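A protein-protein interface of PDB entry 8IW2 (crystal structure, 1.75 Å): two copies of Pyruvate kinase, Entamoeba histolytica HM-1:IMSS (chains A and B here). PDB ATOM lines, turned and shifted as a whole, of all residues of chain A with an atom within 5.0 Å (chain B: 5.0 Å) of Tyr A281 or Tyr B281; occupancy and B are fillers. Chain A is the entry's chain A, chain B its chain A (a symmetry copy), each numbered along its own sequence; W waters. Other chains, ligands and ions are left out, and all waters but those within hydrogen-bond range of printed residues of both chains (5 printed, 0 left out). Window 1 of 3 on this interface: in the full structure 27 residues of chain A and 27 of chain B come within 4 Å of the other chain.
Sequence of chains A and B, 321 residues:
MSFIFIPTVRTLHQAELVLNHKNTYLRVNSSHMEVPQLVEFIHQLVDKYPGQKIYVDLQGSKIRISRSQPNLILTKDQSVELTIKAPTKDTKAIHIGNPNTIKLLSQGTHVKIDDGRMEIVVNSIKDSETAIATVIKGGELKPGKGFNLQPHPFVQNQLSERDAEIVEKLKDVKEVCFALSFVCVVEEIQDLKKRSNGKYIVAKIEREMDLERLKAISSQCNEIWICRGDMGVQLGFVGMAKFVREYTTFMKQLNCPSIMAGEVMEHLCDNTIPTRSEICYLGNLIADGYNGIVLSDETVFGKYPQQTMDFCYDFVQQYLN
Hydrophobic or aromatic side chains of chain B that line the printed part of chain A: Tyr B281.
Along chain B the printed residues that touch a printed residue of chain A span positions 228 to 284.
Of the 13 printed residues of chain A, 6 touch a printed residue of chain B.
Printed residues of chain A that touch a printed residue of chain B: Arg A228, Arg A276, Ser A277, Cys A280, Tyr A281 and Asn A284.
Hydrophobic or aromatic side chains of chain A within 4 Å of the printed part of chain B: Tyr A281.
Arg A228 touches Ser B277, and with the chains exchanged Ser A277 touches Arg B228.
Arg A228 touches Cys B280, and with the chains exchanged Cys A280 touches Arg B228.
Ser A277 touches Tyr B281, and with the chains exchanged Tyr A281 touches Ser B277.
Tyr A281 touches Asn B284, and with the chains exchanged Asn A284 touches Tyr B281.
13 positions are printed for both chains.
The guanidinium group (NH2) of Arg B228 lies within hydrogen-bond range of the side-chain hydroxyl (OG) of Ser A277 (2.8 Å).
The guanidinium group (NE) of Arg A276 sits at hydrogen-bond distance from the backbone carbonyl oxygen (O) of Arg B228, at 2.9 Å.
The guanidinium group (NH2) of Arg A228 is in hydrogen-bond range of the side-chain hydroxyl (OG) of Ser B277.
The backbone carbonyl oxygen (O) of Arg A228 lies within hydrogen-bond range of the guanidinium group (NE) of Arg B276, at 2.9 Å.
Of the printed residues of chain B, Arg A228 touches Arg B276, Ser B277 and Cys B280.
Met A260 touches none of the printed residues of chain B.
Of the printed residues of chain B, Tyr A281 touches Ser B277, Cys B280, Tyr B281 and Asn B284.
Of the printed residues of chain A, Arg B228 touches Arg A276, Ser A277 and Cys A280.
Of the printed residues of chain A, Tyr B281 touches Ser A277, Cys A280, Tyr A281 and Asn A284.
Gly B283 touches none of the printed residues of chain A.
The nearest printed residue of chain B that does not touch Tyr A281 is Arg B276 (5.6 Å).
The nearest printed residue of chain A that does not touch Tyr B281 is Arg A276 (5.6 Å).
The nearest printed residue of chain B that does not touch Ser A277 is Glu B278 (4.5 Å).
Water W5 lies within hydrogen-bond range of OH of Tyr A281 (2.7 Å) and ND2 of Asn B284 (3.1 Å).
Water W4 bridges the side-chain hydroxyl of Tyr B281 (2.7 Å) and the side-chain amide nitrogen of Asn A284 (3.1 Å).
Water W2 bridges OG of Ser B277 (2.8 Å) and O of Glu A278 (2.9 Å).
Water W3 lies within hydrogen-bond range of OG of Ser A277 and O of Glu B278.
Water W1 bridges the side-chain amide nitrogen (ND2) of Asn A284 (3.2 Å) and the side-chain amide nitrogen (ND2) of Asn B284 (3.2 Å).
Among the printed residues, pairs that only touch across the chains: Arg A228 with Cys B280, Ser A277 with Tyr B281, Cys A280 with Arg B228, Cys A280 with Tyr B281, Tyr A281 with Ser B277, Tyr A281 with Cys B280, Tyr A281 with Tyr B281, Tyr A281 with Asn B284 and Asn A284 with Tyr B281.
The side-chain sulfur (SD) of Met A260 sits close to the guanidinium group (NE) of Arg A228, 3.7 Å away.
O of Cys A280 sits close to OD1 of Asn A284 (3.2 Å).
SG of Cys A280 lies within hydrogen-bond range of O of Arg A276, at 3.4 Å.
The guanidinium group of Arg B228 lies close to the side-chain sulfur of Met B260, at 3.7 Å.
The side-chain sulfur (SG) of Cys B280 is in hydrogen-bond range of the backbone carbonyl oxygen (O) of Arg B276 (3.4 Å).
NH1 of Arg A228 is in hydrogen-bond range of OH of Tyr A281.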
ATOM      1  N   ARG A 228     -17.970 -26.230 -14.065  1.00  0.00           N
ATOM      2  CA  ARG A 228     -18.787 -25.660 -15.131  1.00  0.00           C
ATOM      3  C   ARG A 228     -18.855 -26.552 -16.378  1.00  0.00           C
ATOM      4  O   ARG A 228     -19.709 -26.330 -17.212  1.00  0.00           O
ATOM      5  CB  ARG A 228     -18.184 -24.308 -15.472  1.00  0.00           C
ATOM      6  CG  ARG A 228     -18.321 -23.318 -14.310  1.00  0.00           C
ATOM      7  CD  ARG A 228     -17.857 -21.926 -14.686  1.00  0.00           C
ATOM      8  NE  ARG A 228     -16.452 -21.898 -15.092  1.00  0.00           N
ATOM      9  CZ  ARG A 228     -15.884 -20.850 -15.707  1.00  0.00           C
ATOM     10  NH1 ARG A 228     -16.492 -19.670 -15.685  1.00  0.00           N
ATOM     11  NH2 ARG A 228     -14.711 -20.990 -16.324  1.00  0.00           N
ATOM     12  N   VAL A 244     -24.019 -20.201 -11.375  1.00  0.00           N
ATOM     13  CA  VAL A 244     -22.716 -19.838 -10.832  1.00  0.00           C
ATOM     14  C   VAL A 244     -22.775 -18.462 -10.172  1.00  0.00           C
ATOM     15  O   VAL A 244     -22.128 -18.241  -9.174  1.00  0.00           O
ATOM     16  CB  VAL A 244     -21.636 -19.844 -11.935  1.00  0.00           C
ATOM     17  CG1 VAL A 244     -20.289 -19.463 -11.316  1.00  0.00           C
ATOM     18  CG2 VAL A 244     -21.528 -21.205 -12.536  1.00  0.00           C
ATOM     19  N   MET A 260     -13.133 -22.536  -8.436  1.00  0.00           N
ATOM     20  CA  MET A 260     -13.807 -22.456  -9.706  1.00  0.00           C
ATOM     21  C   MET A 260     -13.168 -23.429 -10.677  1.00  0.00           C
ATOM     22  O   MET A 260     -11.947 -23.502 -10.760  1.00  0.00           O
ATOM     23  CB  MET A 260     -13.664 -21.033 -10.258  1.00  0.00           C
ATOM     24  CG  MET A 260     -14.353 -20.821 -11.618  1.00  0.00           C
ATOM     25  SD  MET A 260     -16.284 -20.992 -11.475  1.00  0.00           S
ATOM     26  CE  MET A 260     -16.644 -19.485 -10.450  1.00  0.00           C
ATOM     27  N   ARG A 276      -9.867 -11.415 -23.495  1.00  0.00           N
ATOM     28  CA  ARG A 276     -10.096 -10.350 -22.531  1.00  0.00           C
ATOM     29  C   ARG A 276     -11.181 -10.793 -21.550  1.00  0.00           C
ATOM     30  O   ARG A 276     -11.115 -10.349 -20.420  1.00  0.00           O
ATOM     31  CB  ARG A 276     -10.516  -9.041 -23.206  1.00  0.00           C
ATOM     32  CG  ARG A 276      -9.478  -8.450 -24.155  1.00  0.00           C
ATOM     33  CD  ARG A 276      -8.169  -8.297 -23.462  1.00  0.00           C
ATOM     34  NE  ARG A 276      -7.346  -7.313 -24.138  1.00  0.00           N
ATOM     35  CZ  ARG A 276      -6.125  -7.541 -24.613  1.00  0.00           C
ATOM     36  NH1 ARG A 276      -5.541  -8.735 -24.461  1.00  0.00           N
ATOM     37  NH2 ARG A 276      -5.465  -6.540 -25.162  1.00  0.00           N
ATOM     38  N   SER A 277     -12.180 -11.569 -21.971  1.00  0.00           N
ATOM     39  CA  SER A 277     -13.192 -12.055 -21.011  1.00  0.00           C
ATOM     40  C   SER A 277     -12.593 -13.087 -20.042  1.00  0.00           C
ATOM     41  O   SER A 277     -12.900 -13.081 -18.854  1.00  0.00           O
ATOM     42  CB  SER A 277     -14.446 -12.629 -21.677  1.00  0.00           C
ATOM     43  OG  SER A 277     -15.263 -11.630 -22.173  1.00  0.00           O
ATOM     44  N   GLU A 278     -11.748 -14.013 -20.519  1.00  0.00           N
ATOM     45  CA  GLU A 278     -11.059 -14.900 -19.599  1.00  0.00           C
ATOM     46  C   GLU A 278     -10.350 -14.128 -18.479  1.00  0.00           C
ATOM     47  O   GLU A 278     -10.413 -14.514 -17.297  1.00  0.00           O
ATOM     48  CB  GLU A 278     -10.054 -15.771 -20.358  1.00  0.00           C
ATOM     49  CG  GLU A 278     -10.793 -16.844 -21.149  1.00  0.00           C
ATOM     50  CD  GLU A 278      -9.878 -17.770 -21.910  1.00  0.00           C
ATOM     51  OE1 GLU A 278      -8.843 -17.240 -22.406  1.00  0.00           O
ATOM     52  OE2 GLU A 278     -10.124 -19.030 -21.898  1.00  0.00           O
ATOM     53  N   ILE A 279      -9.587 -13.072 -18.866  1.00  0.00           N
ATOM     54  CA  ILE A 279      -8.764 -12.278 -17.967  1.00  0.00           C
ATOM     55  C   ILE A 279      -9.634 -11.525 -16.959  1.00  0.00           C
ATOM     56  O   ILE A 279      -9.387 -11.565 -15.780  1.00  0.00           O
ATOM     57  CB  ILE A 279      -7.847 -11.338 -18.766  1.00  0.00           C
ATOM     58  CG1 ILE A 279      -6.841 -12.126 -19.619  1.00  0.00           C
ATOM     59  CG2 ILE A 279      -7.171 -10.398 -17.791  1.00  0.00           C
ATOM     60  CD1 ILE A 279      -6.234 -11.314 -20.783  1.00  0.00           C
ATOM     61  N   CYS A 280     -10.666 -10.823 -17.442  1.00  0.00           N
ATOM     62  CA  CYS A 280     -11.583 -10.093 -16.605  1.00  0.00           C
ATOM     63  C   CYS A 280     -12.310 -11.032 -15.659  1.00  0.00           C
ATOM     64  O   CYS A 280     -12.583 -10.690 -14.498  1.00  0.00           O
ATOM     65  CB  CYS A 280     -12.564  -9.268 -17.447  1.00  0.00           C
ATOM     66  SG  CYS A 280     -11.759  -7.819 -18.183  1.00  0.00           S
ATOM     67  N   TYR A 281     -12.762 -12.186 -16.158  1.00  0.00           N
ATOM     68  CA  TYR A 281     -13.470 -13.161 -15.344  1.00  0.00           C
ATOM     69  C   TYR A 281     -12.591 -13.733 -14.234  1.00  0.00           C
ATOM     70  O   TYR A 281     -13.057 -13.879 -13.085  1.00  0.00           O
ATOM     71  CB  TYR A 281     -13.986 -14.293 -16.244  1.00  0.00           C
ATOM     72  CG  TYR A 281     -14.911 -15.237 -15.530  1.00  0.00           C
ATOM     73  CD1 TYR A 281     -16.270 -14.977 -15.521  1.00  0.00           C
ATOM     74  CD2 TYR A 281     -14.448 -16.330 -14.823  1.00  0.00           C
ATOM     75  CE1 TYR A 281     -17.152 -15.816 -14.853  1.00  0.00           C
ATOM     76  CE2 TYR A 281     -15.298 -17.167 -14.123  1.00  0.00           C
ATOM     77  CZ  TYR A 281     -16.662 -16.915 -14.162  1.00  0.00           C
ATOM     78  OH  TYR A 281     -17.491 -17.766 -13.468  1.00  0.00           O
ATOM     79  N   LEU A 282     -11.295 -13.926 -14.529  1.00  0.00           N
ATOM     80  CA  LEU A 282     -10.388 -14.413 -13.495  1.00  0.00           C
ATOM     81  C   LEU A 282     -10.130 -13.331 -12.427  1.00  0.00           C
ATOM     82  O   LEU A 282     -10.222 -13.608 -11.250  1.00  0.00           O
ATOM     83  CB  LEU A 282      -9.104 -14.908 -14.133  1.00  0.00           C
ATOM     84  CG  LEU A 282      -7.989 -15.291 -13.169  1.00  0.00           C
ATOM     85  CD1 LEU A 282      -8.416 -16.425 -12.307  1.00  0.00           C
ATOM     86  CD2 LEU A 282      -6.680 -15.594 -13.925  1.00  0.00           C
ATOM     87  N   GLY A 283     -10.011 -12.066 -12.843  1.00  0.00           N
ATOM     88  CA  GLY A 283      -9.902 -11.008 -11.869  1.00  0.00           C
ATOM     89  C   GLY A 283     -11.149 -10.919 -10.995  1.00  0.00           C
ATOM     90  O   GLY A 283     -11.036 -10.797  -9.793  1.00  0.00           O
ATOM     91  N   ASN A 284     -12.344 -11.014 -11.586  1.00  0.00           N
ATOM     92  CA  ASN A 284     -13.594 -10.891 -10.870  1.00  0.00           C
ATOM     93  C   ASN A 284     -13.790 -12.032  -9.902  1.00  0.00           C
ATOM     94  O   ASN A 284     -14.363 -11.854  -8.803  1.00  0.00           O
ATOM     95  CB  ASN A 284     -14.769 -10.755 -11.827  1.00  0.00           C
ATOM     96  CG  ASN A 284     -14.728  -9.486 -12.680  1.00  0.00           C
ATOM     97  OD1 ASN A 284     -13.895  -8.631 -12.461  1.00  0.00           O
ATOM     98  ND2 ASN A 284     -15.594  -9.402 -13.655  1.00  0.00           N
ATOM     99  N   LEU A 285     -13.367 -13.231 -10.262  1.00  0.00           N
ATOM    100  CA  LEU A 285     -13.524 -14.349  -9.335  1.00  0.00           C
ATOM    101  C   LEU A 285     -12.570 -14.238  -8.114  1.00  0.00           C
ATOM    102  O   LEU A 285     -12.961 -14.579  -6.962  1.00  0.00           O
ATOM    103  CB  LEU A 285     -13.495 -15.707 -10.071  1.00  0.00           C
ATOM    104  CG  LEU A 285     -12.196 -16.232 -10.530  1.00  0.00           C
ATOM    105  CD1 LEU A 285     -11.407 -16.819  -9.348  1.00  0.00           C
ATOM    106  CD2 LEU A 285     -12.391 -17.274 -11.649  1.00  0.00           C
ATOM    107  N   ARG B 228     -11.901  -3.168 -24.270  1.00  0.00           N
ATOM    108  CA  ARG B 228     -10.890  -3.948 -23.565  1.00  0.00           C
ATOM    109  C   ARG B 228      -9.679  -4.297 -24.441  1.00  0.00           C
ATOM    110  O   ARG B 228      -8.664  -4.694 -23.907  1.00  0.00           O
ATOM    111  CB  ARG B 228     -11.575  -5.211 -23.071  1.00  0.00           C
ATOM    112  CG  ARG B 228     -12.635  -4.902 -22.008  1.00  0.00           C
ATOM    113  CD  ARG B 228     -13.223  -6.159 -21.402  1.00  0.00           C
ATOM    114  NE  ARG B 228     -13.872  -7.008 -22.401  1.00  0.00           N
ATOM    115  CZ  ARG B 228     -14.236  -8.276 -22.165  1.00  0.00           C
ATOM    116  NH1 ARG B 228     -14.313  -8.713 -20.913  1.00  0.00           N
ATOM    117  NH2 ARG B 228     -14.531  -9.090 -23.180  1.00  0.00           N
ATOM    118  N   VAL B 244     -12.100  -2.414 -15.351  1.00  0.00           N
ATOM    119  CA  VAL B 244     -13.439  -2.740 -15.828  1.00  0.00           C
ATOM    120  C   VAL B 244     -14.367  -3.044 -14.654  1.00  0.00           C
ATOM    121  O   VAL B 244     -15.528  -2.707 -14.697  1.00  0.00           O
ATOM    122  CB  VAL B 244     -13.405  -3.942 -16.794  1.00  0.00           C
ATOM    123  CG1 VAL B 244     -14.829  -4.239 -17.271  1.00  0.00           C
ATOM    124  CG2 VAL B 244     -12.553  -3.623 -17.977  1.00  0.00           C
ATOM    125  N   MET B 260     -20.159  -3.149 -23.544  1.00  0.00           N
ATOM    126  CA  MET B 260     -18.918  -3.845 -23.328  1.00  0.00           C
ATOM    127  C   MET B 260     -18.313  -4.221 -24.667  1.00  0.00           C
ATOM    128  O   MET B 260     -19.017  -4.709 -25.544  1.00  0.00           O
ATOM    129  CB  MET B 260     -19.194  -5.123 -22.529  1.00  0.00           C
ATOM    130  CG  MET B 260     -17.934  -5.955 -22.229  1.00  0.00           C
ATOM    131  SD  MET B 260     -16.717  -5.008 -21.045  1.00  0.00           S
ATOM    132  CE  MET B 260     -17.742  -5.012 -19.496  1.00  0.00           C
ATOM    133  N   ARG B 276     -16.614 -21.662 -21.139  1.00  0.00           N
ATOM    134  CA  ARG B 276     -17.512 -21.503 -20.007  1.00  0.00           C
ATOM    135  C   ARG B 276     -17.290 -20.124 -19.387  1.00  0.00           C
ATOM    136  O   ARG B 276     -18.250 -19.598 -18.857  1.00  0.00           O
ATOM    137  CB  ARG B 276     -17.301 -22.586 -18.946  1.00  0.00           C
ATOM    138  CG  ARG B 276     -17.572 -24.010 -19.422  1.00  0.00           C
ATOM    139  CD  ARG B 276     -18.932 -24.107 -20.019  1.00  0.00           C
ATOM    140  NE  ARG B 276     -19.396 -25.481 -20.010  1.00  0.00           N
ATOM    141  CZ  ARG B 276     -19.782 -26.159 -21.088  1.00  0.00           C
ATOM    142  NH1 ARG B 276     -19.798 -25.581 -22.293  1.00  0.00           N
ATOM    143  NH2 ARG B 276     -20.231 -27.389 -20.930  1.00  0.00           N
ATOM    144  N   SER B 277     -16.068 -19.590 -19.378  1.00  0.00           N
ATOM    145  CA  SER B 277     -15.862 -18.229 -18.841  1.00  0.00           C
ATOM    146  C   SER B 277     -16.490 -17.166 -19.757  1.00  0.00           C
ATOM    147  O   SER B 277     -17.079 -16.200 -19.281  1.00  0.00           O
ATOM    148  CB  SER B 277     -14.393 -17.889 -18.575  1.00  0.00           C
ATOM    149  OG  SER B 277     -13.924 -18.510 -17.434  1.00  0.00           O
ATOM    150  N   GLU B 278     -16.364 -17.295 -21.086  1.00  0.00           N
ATOM    151  CA  GLU B 278     -17.073 -16.386 -21.968  1.00  0.00           C
ATOM    152  C   GLU B 278     -18.567 -16.306 -21.629  1.00  0.00           C
ATOM    153  O   GLU B 278     -19.157 -15.210 -21.597  1.00  0.00           O
ATOM    154  CB  GLU B 278     -16.884 -16.810 -23.427  1.00  0.00           C
ATOM    155  CG  GLU B 278     -15.472 -16.468 -23.886  1.00  0.00           C
ATOM    156  CD  GLU B 278     -15.202 -16.828 -25.326  1.00  0.00           C
ATOM    157  OE1 GLU B 278     -15.747 -17.890 -25.742  1.00  0.00           O
ATOM    158  OE2 GLU B 278     -14.566 -15.992 -26.064  1.00  0.00           O
ATOM    159  N   ILE B 279     -19.210 -17.491 -21.464  1.00  0.00           N
ATOM    160  CA  ILE B 279     -20.641 -17.626 -21.234  1.00  0.00           C
ATOM    161  C   ILE B 279     -21.035 -17.006 -19.893  1.00  0.00           C
ATOM    162  O   ILE B 279     -21.957 -16.233 -19.818  1.00  0.00           O
ATOM    163  CB  ILE B 279     -21.066 -19.098 -21.348  1.00  0.00           C
ATOM    164  CG1 ILE B 279     -20.849 -19.639 -22.769  1.00  0.00           C
ATOM    165  CG2 ILE B 279     -22.509 -19.207 -20.899  1.00  0.00           C
ATOM    166  CD1 ILE B 279     -20.784 -21.179 -22.851  1.00  0.00           C
ATOM    167  N   CYS B 280     -20.321 -17.363 -18.818  1.00  0.00           N
ATOM    168  CA  CYS B 280     -20.564 -16.834 -17.501  1.00  0.00           C
ATOM    169  C   CYS B 280     -20.358 -15.330 -17.480  1.00  0.00           C
ATOM    170  O   CYS B 280     -21.080 -14.592 -16.791  1.00  0.00           O
ATOM    171  CB  CYS B 280     -19.694 -17.539 -16.453  1.00  0.00           C
ATOM    172  SG  CYS B 280     -20.286 -19.219 -16.113  1.00  0.00           S
ATOM    173  N   TYR B 281     -19.292 -14.842 -18.121  1.00  0.00           N
ATOM    174  CA  TYR B 281     -18.997 -13.419 -18.168  1.00  0.00           C
ATOM    175  C   TYR B 281     -20.076 -12.630 -18.907  1.00  0.00           C
ATOM    176  O   TYR B 281     -20.477 -11.543 -18.444  1.00  0.00           O
ATOM    177  CB  TYR B 281     -17.634 -13.206 -18.842  1.00  0.00           C
ATOM    178  CG  TYR B 281     -17.145 -11.789 -18.746  1.00  0.00           C
ATOM    179  CD1 TYR B 281     -16.375 -11.410 -17.661  1.00  0.00           C
ATOM    180  CD2 TYR B 281     -17.488 -10.826 -19.675  1.00  0.00           C
ATOM    181  CE1 TYR B 281     -15.923 -10.104 -17.528  1.00  0.00           C
ATOM    182  CE2 TYR B 281     -17.080  -9.510 -19.555  1.00  0.00           C
ATOM    183  CZ  TYR B 281     -16.271  -9.158 -18.483  1.00  0.00           C
ATOM    184  OH  TYR B 281     -15.867  -7.847 -18.388  1.00  0.00           O
ATOM    185  N   LEU B 282     -20.642 -13.228 -19.967  1.00  0.00           N
ATOM    186  CA  LEU B 282     -21.721 -12.555 -20.680  1.00  0.00           C
ATOM    187  C   LEU B 282     -23.011 -12.518 -19.834  1.00  0.00           C
ATOM    188  O   LEU B 282     -23.621 -11.479 -19.705  1.00  0.00           O
ATOM    189  CB  LEU B 282     -21.937 -13.219 -22.027  1.00  0.00           C
ATOM    190  CG  LEU B 282     -23.146 -12.735 -22.819  1.00  0.00           C
ATOM    191  CD1 LEU B 282     -23.002 -11.294 -23.154  1.00  0.00           C
ATOM    192  CD2 LEU B 282     -23.373 -13.606 -24.072  1.00  0.00           C
ATOM    193  N   GLY B 283     -23.300 -13.598 -19.101  1.00  0.00           N
ATOM    194  CA  GLY B 283     -24.421 -13.557 -18.194  1.00  0.00           C
ATOM    195  C   GLY B 283     -24.229 -12.502 -17.109  1.00  0.00           C
ATOM    196  O   GLY B 283     -25.142 -11.756 -16.825  1.00  0.00           O
ATOM    197  N   ASN B 284     -23.031 -12.410 -16.522  1.00  0.00           N
ATOM    198  CA  ASN B 284     -22.745 -11.486 -15.447  1.00  0.00           C
ATOM    199  C   ASN B 284     -22.818 -10.053 -15.916  1.00  0.00           C
ATOM    200  O   ASN B 284     -23.242  -9.149 -15.162  1.00  0.00           O
ATOM    201  CB  ASN B 284     -21.409 -11.798 -14.791  1.00  0.00           C
ATOM    202  CG  ASN B 284     -21.361 -13.162 -14.102  1.00  0.00           C
ATOM    203  OD1 ASN B 284     -22.373 -13.824 -13.990  1.00  0.00           O
ATOM    204  ND2 ASN B 284     -20.192 -13.576 -13.691  1.00  0.00           N
ATOM    205  N   LEU B 285     -22.390  -9.777 -17.136  1.00  0.00           N
ATOM    206  CA  LEU B 285     -22.470  -8.403 -17.624  1.00  0.00           C
ATOM    207  C   LEU B 285     -23.934  -7.960 -17.898  1.00  0.00           C
ATOM    208  O   LEU B 285     -24.310  -6.786 -17.623  1.00  0.00           O
ATOM    209  CB  LEU B 285     -21.480  -8.151 -18.782  1.00  0.00           C
ATOM    210  CG  LEU B 285     -21.811  -8.676 -20.120  1.00  0.00           C
ATOM    211  CD1 LEU B 285     -22.874  -7.792 -20.793  1.00  0.00           C
ATOM    212  CD2 LEU B 285     -20.545  -8.797 -20.990  1.00  0.00           C
HETATM  213  O   HOH W   1     -17.598 -11.809 -14.220  1.00  0.00           O
HETATM  214  O   HOH W   2     -11.564 -17.156 -16.800  1.00  0.00           O
HETATM  215  O   HOH W   3     -17.724 -12.874 -22.617  1.00  0.00           O
HETATM  216  O   HOH W   4     -15.362  -7.228 -15.786  1.00  0.00           O
HETATM  217  O   HOH W   5     -19.773 -16.456 -12.769  1.00  0.00           O
